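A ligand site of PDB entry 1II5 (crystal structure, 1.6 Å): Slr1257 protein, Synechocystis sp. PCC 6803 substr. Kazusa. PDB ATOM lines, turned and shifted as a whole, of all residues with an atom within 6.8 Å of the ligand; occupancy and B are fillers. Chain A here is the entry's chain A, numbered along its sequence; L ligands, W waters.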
ATOM      1  N   VAL A  11      -0.458  29.378  17.078  1.00  0.00           N
ATOM      2  CA  VAL A  11      -1.275  29.415  18.281  1.00  0.00           C
ATOM      3  C   VAL A  11      -0.473  30.118  19.388  1.00  0.00           C
ATOM      4  O   VAL A  11       0.752  30.174  19.328  1.00  0.00           O
ATOM      5  CB  VAL A  11      -1.662  27.976  18.703  1.00  0.00           C
ATOM      6  CG1 VAL A  11      -0.440  27.223  19.222  1.00  0.00           C
ATOM      7  CG2 VAL A  11      -2.771  28.006  19.725  1.00  0.00           C
ATOM      8  N   GLY A  12      -1.167  30.707  20.362  1.00  0.00           N
ATOM      9  CA  GLY A  12      -0.468  31.386  21.436  1.00  0.00           C
ATOM     10  C   GLY A  12      -0.880  32.832  21.635  1.00  0.00           C
ATOM     11  O   GLY A  12      -1.675  33.372  20.871  1.00  0.00           O
ATOM     12  N   ASN A  13      -0.275  33.465  22.637  1.00  0.00           N
ATOM     13  CA  ASN A  13      -0.586  34.857  22.996  1.00  0.00           C
ATOM     14  C   ASN A  13       0.657  35.735  23.039  1.00  0.00           C
ATOM     15  O   ASN A  13       1.779  35.238  22.956  1.00  0.00           O
ATOM     16  CB  ASN A  13      -1.225  34.872  24.392  1.00  0.00           C
ATOM     17  CG  ASN A  13      -2.583  34.198  24.426  1.00  0.00           C
ATOM     18  OD1 ASN A  13      -3.610  34.860  24.337  1.00  0.00           O
ATOM     19  ND2 ASN A  13      -2.582  32.864  24.533  1.00  0.00           N
ATOM     20  N   PRO A  14       0.462  37.071  23.118  1.00  0.00           N
ATOM     21  CA  PRO A  14       1.573  38.028  23.178  1.00  0.00           C
ATOM     22  C   PRO A  14       2.429  37.758  24.410  1.00  0.00           C
ATOM     23  O   PRO A  14       1.917  37.344  25.447  1.00  0.00           O
ATOM     24  CB  PRO A  14       0.836  39.362  23.314  1.00  0.00           C
ATOM     25  CG  PRO A  14      -0.392  39.147  22.519  1.00  0.00           C
ATOM     26  CD  PRO A  14      -0.823  37.786  22.992  1.00  0.00           C
ATOM     27  N   PHE A  16       4.595  36.342  22.340  1.00  0.00           N
ATOM     28  CA  PHE A  16       5.065  35.298  21.436  1.00  0.00           C
ATOM     29  C   PHE A  16       4.297  35.243  20.119  1.00  0.00           C
ATOM     30  O   PHE A  16       4.885  35.010  19.056  1.00  0.00           O
ATOM     31  CB  PHE A  16       5.088  33.946  22.156  1.00  0.00           C
ATOM     32  CG  PHE A  16       6.244  33.814  23.104  1.00  0.00           C
ATOM     33  CD1 PHE A  16       6.146  34.229  24.426  1.00  0.00           C
ATOM     34  CD2 PHE A  16       7.475  33.341  22.642  1.00  0.00           C
ATOM     35  CE1 PHE A  16       7.259  34.198  25.282  1.00  0.00           C
ATOM     36  CE2 PHE A  16       8.599  33.299  23.491  1.00  0.00           C
ATOM     37  CZ  PHE A  16       8.480  33.740  24.809  1.00  0.00           C
ATOM     38  N   VAL A  17       3.007  35.523  20.180  1.00  0.00           N
ATOM     39  CA  VAL A  17       2.154  35.523  19.000  1.00  0.00           C
ATOM     40  C   VAL A  17       1.115  36.642  19.105  1.00  0.00           C
ATOM     41  O   VAL A  17       0.481  36.802  20.149  1.00  0.00           O
ATOM     42  CB  VAL A  17       1.410  34.175  18.815  1.00  0.00           C
ATOM     43  CG1 VAL A  17       0.413  34.285  17.668  1.00  0.00           C
ATOM     44  CG2 VAL A  17       2.396  33.050  18.538  1.00  0.00           C
ATOM     45  N   ILE A  54      -3.816  24.504  21.188  1.00  0.00           N
ATOM     46  CA  ILE A  54      -2.607  23.721  20.998  1.00  0.00           C
ATOM     47  C   ILE A  54      -2.977  22.282  20.649  1.00  0.00           C
ATOM     48  O   ILE A  54      -2.404  21.700  19.740  1.00  0.00           O
ATOM     49  CB  ILE A  54      -1.698  23.787  22.256  1.00  0.00           C
ATOM     50  CG1 ILE A  54      -1.104  25.187  22.363  1.00  0.00           C
ATOM     51  CG2 ILE A  54      -0.595  22.749  22.184  1.00  0.00           C
ATOM     52  CD1 ILE A  54      -0.345  25.457  23.653  1.00  0.00           C
ATOM     53  N   PRO A  72       4.282  29.605  21.546  1.00  0.00           N
ATOM     54  CA  PRO A  72       4.847  29.350  22.879  1.00  0.00           C
ATOM     55  C   PRO A  72       4.254  28.047  23.410  1.00  0.00           C
ATOM     56  O   PRO A  72       3.519  28.032  24.405  1.00  0.00           O
ATOM     57  CB  PRO A  72       4.381  30.568  23.668  1.00  0.00           C
ATOM     58  CG  PRO A  72       3.042  30.852  23.081  1.00  0.00           C
ATOM     59  CD  PRO A  72       3.281  30.697  21.598  1.00  0.00           C
ATOM     60  N   ILE A  73       4.567  26.948  22.732  1.00  0.00           N
ATOM     61  CA  ILE A  73       4.045  25.631  23.079  1.00  0.00           C
ATOM     62  C   ILE A  73       4.918  24.892  24.099  1.00  0.00           C
ATOM     63  O   ILE A  73       6.040  24.474  23.793  1.00  0.00           O
ATOM     64  CB  ILE A  73       3.878  24.770  21.801  1.00  0.00           C
ATOM     65  CG1 ILE A  73       3.097  25.578  20.751  1.00  0.00           C
ATOM     66  CG2 ILE A  73       3.173  23.456  22.110  1.00  0.00           C
ATOM     67  CD1 ILE A  73       3.327  25.140  19.334  1.00  0.00           C
ATOM     68  N   SER A  74       4.408  24.758  25.322  1.00  0.00           N
ATOM     69  CA  SER A  74       5.128  24.059  26.385  1.00  0.00           C
ATOM     70  C   SER A  74       5.354  22.591  26.020  1.00  0.00           C
ATOM     71  O   SER A  74       4.432  21.916  25.548  1.00  0.00           O
ATOM     72  CB  SER A  74       4.357  24.139  27.701  1.00  0.00           C
ATOM     73  OG  SER A  74       4.243  25.480  28.138  1.00  0.00           O
ATOM     74  N   VAL A  75       6.593  22.126  26.180  1.00  0.00           N
ATOM     75  CA  VAL A  75       6.956  20.747  25.906  1.00  0.00           C
ATOM     76  C   VAL A  75       6.631  19.971  27.181  1.00  0.00           C
ATOM     77  O   VAL A  75       7.328  20.104  28.185  1.00  0.00           O
ATOM     78  CB  VAL A  75       8.465  20.586  25.572  1.00  0.00           C
ATOM     79  CG1 VAL A  75       8.777  19.150  25.169  1.00  0.00           C
ATOM     80  CG2 VAL A  75       8.881  21.545  24.464  1.00  0.00           C
ATOM     81  N   THR A  76       5.561  19.188  27.145  1.00  0.00           N
ATOM     82  CA  THR A  76       5.142  18.402  28.302  1.00  0.00           C
ATOM     83  C   THR A  76       5.101  16.925  27.959  1.00  0.00           C
ATOM     84  O   THR A  76       5.008  16.563  26.774  1.00  0.00           O
ATOM     85  CB  THR A  76       3.721  18.798  28.759  1.00  0.00           C
ATOM     86  OG1 THR A  76       2.778  18.445  27.741  1.00  0.00           O
ATOM     87  CG2 THR A  76       3.630  20.296  29.020  1.00  0.00           C
ATOM     88  N   ARG A  79       1.991  15.876  25.996  1.00  0.00           N
ATOM     89  CA  ARG A  79       2.011  16.283  24.596  1.00  0.00           C
ATOM     90  C   ARG A  79       3.019  15.473  23.782  1.00  0.00           C
ATOM     91  O   ARG A  79       2.756  15.120  22.633  1.00  0.00           O
ATOM     92  CB  ARG A  79       2.284  17.777  24.454  1.00  0.00           C
ATOM     93  CG  ARG A  79       1.132  18.621  24.945  1.00  0.00           C
ATOM     94  CD  ARG A  79       1.428  20.080  24.829  1.00  0.00           C
ATOM     95  NE  ARG A  79       0.333  20.862  25.416  1.00  0.00           N
ATOM     96  CZ  ARG A  79       0.456  22.126  25.794  1.00  0.00           C
ATOM     97  NH1 ARG A  79       1.619  22.739  25.645  1.00  0.00           N
ATOM     98  NH2 ARG A  79      -0.590  22.773  26.285  1.00  0.00           N
ATOM     99  N   SER A  94      10.421  29.216  29.735  1.00  0.00           N
ATOM    100  CA  SER A  94       9.423  30.067  30.345  1.00  0.00           C
ATOM    101  C   SER A  94       8.974  29.580  31.707  1.00  0.00           C
ATOM    102  O   SER A  94       9.394  28.523  32.170  1.00  0.00           O
ATOM    103  CB  SER A  94       8.212  30.170  29.409  1.00  0.00           C
ATOM    104  OG  SER A  94       7.316  31.185  29.818  1.00  0.00           O
ATOM    105  N   ILE A  96       5.478  29.531  34.503  1.00  0.00           N
ATOM    106  CA  ILE A  96       4.051  29.727  34.634  1.00  0.00           C
ATOM    107  C   ILE A  96       3.892  30.553  35.917  1.00  0.00           C
ATOM    108  O   ILE A  96       4.427  30.185  36.948  1.00  0.00           O
ATOM    109  CB  ILE A  96       3.319  28.366  34.731  1.00  0.00           C
ATOM    110  CG1 ILE A  96       3.652  27.512  33.498  1.00  0.00           C
ATOM    111  CG2 ILE A  96       1.815  28.556  34.847  1.00  0.00           C
ATOM    112  CD1 ILE A  96       3.468  28.209  32.164  1.00  0.00           C
ATOM    113  N   VAL A 122      -6.790  29.772  31.362  1.00  0.00           N
ATOM    114  CA  VAL A 122      -7.259  29.727  29.974  1.00  0.00           C
ATOM    115  C   VAL A 122      -7.316  28.257  29.560  1.00  0.00           C
ATOM    116  O   VAL A 122      -6.401  27.489  29.841  1.00  0.00           O
ATOM    117  CB  VAL A 122      -6.314  30.528  29.025  1.00  0.00           C
ATOM    118  CG1 VAL A 122      -6.807  30.448  27.593  1.00  0.00           C
ATOM    119  CG2 VAL A 122      -6.262  31.985  29.466  1.00  0.00           C
ATOM    120  N   ASP A 124      -7.123  24.720  27.684  1.00  0.00           N
ATOM    121  CA  ASP A 124      -6.075  24.054  26.894  1.00  0.00           C
ATOM    122  C   ASP A 124      -4.683  24.639  27.054  1.00  0.00           C
ATOM    123  O   ASP A 124      -3.964  24.787  26.081  1.00  0.00           O
ATOM    124  CB  ASP A 124      -6.435  24.006  25.400  1.00  0.00           C
ATOM    125  CG  ASP A 124      -5.626  22.962  24.586  1.00  0.00           C
ATOM    126  OD1 ASP A 124      -4.545  22.469  25.030  1.00  0.00           O
ATOM    127  OD2 ASP A 124      -6.060  22.681  23.443  1.00  0.00           O
ATOM    128  N   THR A 125      -4.338  25.066  28.268  1.00  0.00           N
ATOM    129  CA  THR A 125      -2.988  25.561  28.519  1.00  0.00           C
ATOM    130  C   THR A 125      -2.515  24.721  29.677  1.00  0.00           C
ATOM    131  O   THR A 125      -3.316  24.114  30.387  1.00  0.00           O
ATOM    132  CB  THR A 125      -2.945  27.073  28.886  1.00  0.00           C
ATOM    133  OG1 THR A 125      -3.709  27.308  30.060  1.00  0.00           O
ATOM    134  CG2 THR A 125      -3.477  27.915  27.728  1.00  0.00           C
ATOM    135  N   THR A 126      -1.198  24.644  29.850  1.00  0.00           N
ATOM    136  CA  THR A 126      -0.629  23.852  30.926  1.00  0.00           C
ATOM    137  C   THR A 126      -1.090  24.350  32.293  1.00  0.00           C
ATOM    138  O   THR A 126      -1.138  23.574  33.251  1.00  0.00           O
ATOM    139  CB  THR A 126       0.901  23.837  30.852  1.00  0.00           C
ATOM    140  OG1 THR A 126       1.391  25.183  30.884  1.00  0.00           O
ATOM    141  CG2 THR A 126       1.382  23.148  29.570  1.00  0.00           C
ATOM    142  N   ALA A 127      -1.470  25.625  32.364  1.00  0.00           N
ATOM    143  CA  ALA A 127      -1.942  26.227  33.613  1.00  0.00           C
ATOM    144  C   ALA A 127      -3.165  25.498  34.183  1.00  0.00           C
ATOM    145  O   ALA A 127      -3.338  25.431  35.398  1.00  0.00           O
ATOM    146  CB  ALA A 127      -2.255  27.705  33.415  1.00  0.00           C
ATOM    147  N   PHE A 161      -1.120  31.808  34.360  1.00  0.00           N
ATOM    148  CA  PHE A 161      -0.769  31.754  32.949  1.00  0.00           C
ATOM    149  C   PHE A 161       0.731  31.993  32.805  1.00  0.00           C
ATOM    150  O   PHE A 161       1.409  32.372  33.757  1.00  0.00           O
ATOM    151  CB  PHE A 161      -1.544  32.845  32.205  1.00  0.00           C
ATOM    152  CG  PHE A 161      -1.598  32.665  30.709  1.00  0.00           C
ATOM    153  CD1 PHE A 161      -2.585  31.868  30.130  1.00  0.00           C
ATOM    154  CD2 PHE A 161      -0.700  33.321  29.876  1.00  0.00           C
ATOM    155  CE1 PHE A 161      -2.669  31.745  28.741  1.00  0.00           C
ATOM    156  CE2 PHE A 161      -0.784  33.198  28.487  1.00  0.00           C
ATOM    157  CZ  PHE A 161      -1.776  32.411  27.928  1.00  0.00           C
ATOM    158  N   ASP A 162       1.252  31.746  31.608  1.00  0.00           N
ATOM    159  CA  ASP A 162       2.662  31.938  31.309  1.00  0.00           C
ATOM    160  C   ASP A 162       3.106  33.337  31.730  1.00  0.00           C
ATOM    161  O   ASP A 162       2.494  34.325  31.351  1.00  0.00           O
ATOM    162  CB  ASP A 162       2.905  31.773  29.807  1.00  0.00           C
ATOM    163  CG  ASP A 162       2.497  30.400  29.313  1.00  0.00           C
ATOM    164  OD1 ASP A 162       3.370  29.714  28.736  1.00  0.00           O
ATOM    165  OD2 ASP A 162       1.320  30.019  29.503  1.00  0.00           O
ATOM    166  N   ALA A 165       3.615  36.394  29.147  1.00  0.00           N
ATOM    167  CA  ALA A 165       2.337  36.918  28.657  1.00  0.00           C
ATOM    168  C   ALA A 165       1.675  37.793  29.722  1.00  0.00           C
ATOM    169  O   ALA A 165       1.082  38.820  29.399  1.00  0.00           O
ATOM    170  CB  ALA A 165       1.408  35.785  28.243  1.00  0.00           C
ATOM    171  N   GLU A 188       8.876  25.758  32.231  1.00  0.00           N
ATOM    172  CA  GLU A 188       8.570  24.943  31.070  1.00  0.00           C
ATOM    173  C   GLU A 188       9.259  25.450  29.822  1.00  0.00           C
ATOM    174  O   GLU A 188       9.294  26.647  29.570  1.00  0.00           O
ATOM    175  CB  GLU A 188       7.067  24.966  30.801  1.00  0.00           C
ATOM    176  CG  GLU A 188       6.248  24.386  31.916  1.00  0.00           C
ATOM    177  CD  GLU A 188       4.750  24.597  31.764  1.00  0.00           C
ATOM    178  OE1 GLU A 188       4.280  25.133  30.729  1.00  0.00           O
ATOM    179  OE2 GLU A 188       4.036  24.214  32.702  1.00  0.00           O
ATOM    180  N   PRO A 189       9.791  24.538  29.002  1.00  0.00           N
ATOM    181  CA  PRO A 189      10.463  24.929  27.766  1.00  0.00           C
ATOM    182  C   PRO A 189       9.424  25.049  26.634  1.00  0.00           C
ATOM    183  O   PRO A 189       8.398  24.360  26.667  1.00  0.00           O
ATOM    184  CB  PRO A 189      11.421  23.769  27.527  1.00  0.00           C
ATOM    185  CG  PRO A 189      10.660  22.605  28.016  1.00  0.00           C
ATOM    186  CD  PRO A 189       9.995  23.103  29.284  1.00  0.00           C
ATOM    187  N   TYR A 190       9.639  25.968  25.696  1.00  0.00           N
ATOM    188  CA  TYR A 190       8.750  26.152  24.551  1.00  0.00           C
ATOM    189  C   TYR A 190       9.415  25.530  23.326  1.00  0.00           C
ATOM    190  O   TYR A 190      10.608  25.735  23.112  1.00  0.00           O
ATOM    191  CB  TYR A 190       8.538  27.620  24.185  1.00  0.00           C
ATOM    192  CG  TYR A 190       7.714  28.458  25.119  1.00  0.00           C
ATOM    193  CD1 TYR A 190       7.737  29.841  25.018  1.00  0.00           C
ATOM    194  CD2 TYR A 190       6.894  27.878  26.098  1.00  0.00           C
ATOM    195  CE1 TYR A 190       6.986  30.639  25.846  1.00  0.00           C
ATOM    196  CE2 TYR A 190       6.129  28.683  26.950  1.00  0.00           C
ATOM    197  CZ  TYR A 190       6.192  30.065  26.811  1.00  0.00           C
ATOM    198  OH  TYR A 190       5.480  30.910  27.629  1.00  0.00           O
HETATM  199  N1  LIG L   1       2.705  27.720  27.086  1.00  0.00           N
HETATM  200  C1  LIG L   1       1.236  27.494  27.142  1.00  0.00           C
HETATM  201  C2  LIG L   1       0.946  26.032  26.821  1.00  0.00           C
HETATM  202  O1  LIG L   1       1.794  25.414  26.148  1.00  0.00           O
HETATM  203  C3  LIG L   1       0.509  28.401  26.139  1.00  0.00           C
HETATM  204  C4  LIG L   1       0.792  29.870  26.360  1.00  0.00           C
HETATM  205  C5  LIG L   1       0.056  30.778  25.386  1.00  0.00           C
HETATM  206  O2  LIG L   1      -1.037  30.412  24.898  1.00  0.00           O
HETATM  207  O3  LIG L   1       0.572  31.892  25.114  1.00  0.00           O
HETATM  208  O4  LIG L   1      -0.108  25.518  27.237  1.00  0.00           O
HETATM  209  O   HOH W   1      -2.463  28.546  23.339  1.00  0.00           O
HETATM  210  O   HOH W   2       2.581  33.785  25.349  1.00  0.00           O
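Water W2 bridges O3 of the ligand (2.8 Å) and O of Asn 13 (2.9 Å).
CA of Gly 12 touches O2 of the ligand, 3.6 Å away. CD1 of Ile 54 touches O1 of the ligand, at 3.3 Å. C of Ile 73 touches O1 of the ligand, 3.8 Å away. CA of Thr 125 touches O4 of the ligand (3.2 Å). CZ of Phe 161 touches C5 of the ligand (3.5 Å). Tyr 190 touches the ligand. Hydrophobic or aromatic side chains that line the ligand: Ile 54, Pro 72, Phe 161 and Tyr 190. The nearest printed residue that does not touch the ligand is Asp 124 (4.1 Å).
OG of Ser 94 lies within hydrogen-bond range of OH of Tyr 190 (2.9 Å). The side-chain hydroxyl (OG1) of Thr 125 lies within hydrogen-bond range of the backbone carbonyl oxygen (O) of Val 122 (2.7 Å). OH of Tyr 190 lies within hydrogen-bond range of OD1 of Asp 162, at 2.7 Å. The side-chain carboxylate (OE1) of Glu 188 is in hydrogen-bond range of the side-chain hydroxyl (OG) of Ser 74, 2.6 Å away. OG1 of Thr 126 lies within hydrogen-bond range of OE1 of Glu 188, 2.9 Å away. The side-chain hydroxyl of Thr 76 sits at hydrogen-bond distance from the backbone NH of Arg 79, at 3.2 Å. The guanidinium group (NH1) of Arg 79 sits at hydrogen-bond distance from the backbone carbonyl oxygen (O) of Ser 74 (2.9 Å).
The backbone NH (N) of Thr 126 is in hydrogen-bond range of an oxygen (O4) of the ligand, 3.0 Å away. N1 of the ligand is in hydrogen-bond range of O of Pro 72 (2.8 Å). The side-chain amide nitrogen (ND2) of Asn 13 sits at hydrogen-bond distance from an oxygen (O2) of the ligand (2.9 Å). The side-chain carboxylate (OD1) of Asp 162 is in salt-bridge range of a nitrogen (N1) of the ligand, at 2.7 Å. The side-chain hydroxyl (OG) of Ser 74 is in hydrogen-bond range of a nitrogen (N1) of the ligand (2.9 Å). The guanidinium group (NH1) of Arg 79 is in salt-bridge range of an oxygen (O1) of the ligand, at 2.7 Å. The backbone NH (N) of Ser 74 lies within hydrogen-bond range of an oxygen (O1) of the ligand (2.8 Å). The backbone NH (N) of Asn 13 lies within hydrogen-bond range of an oxygen (O3) of the ligand, at 3.1 Å.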
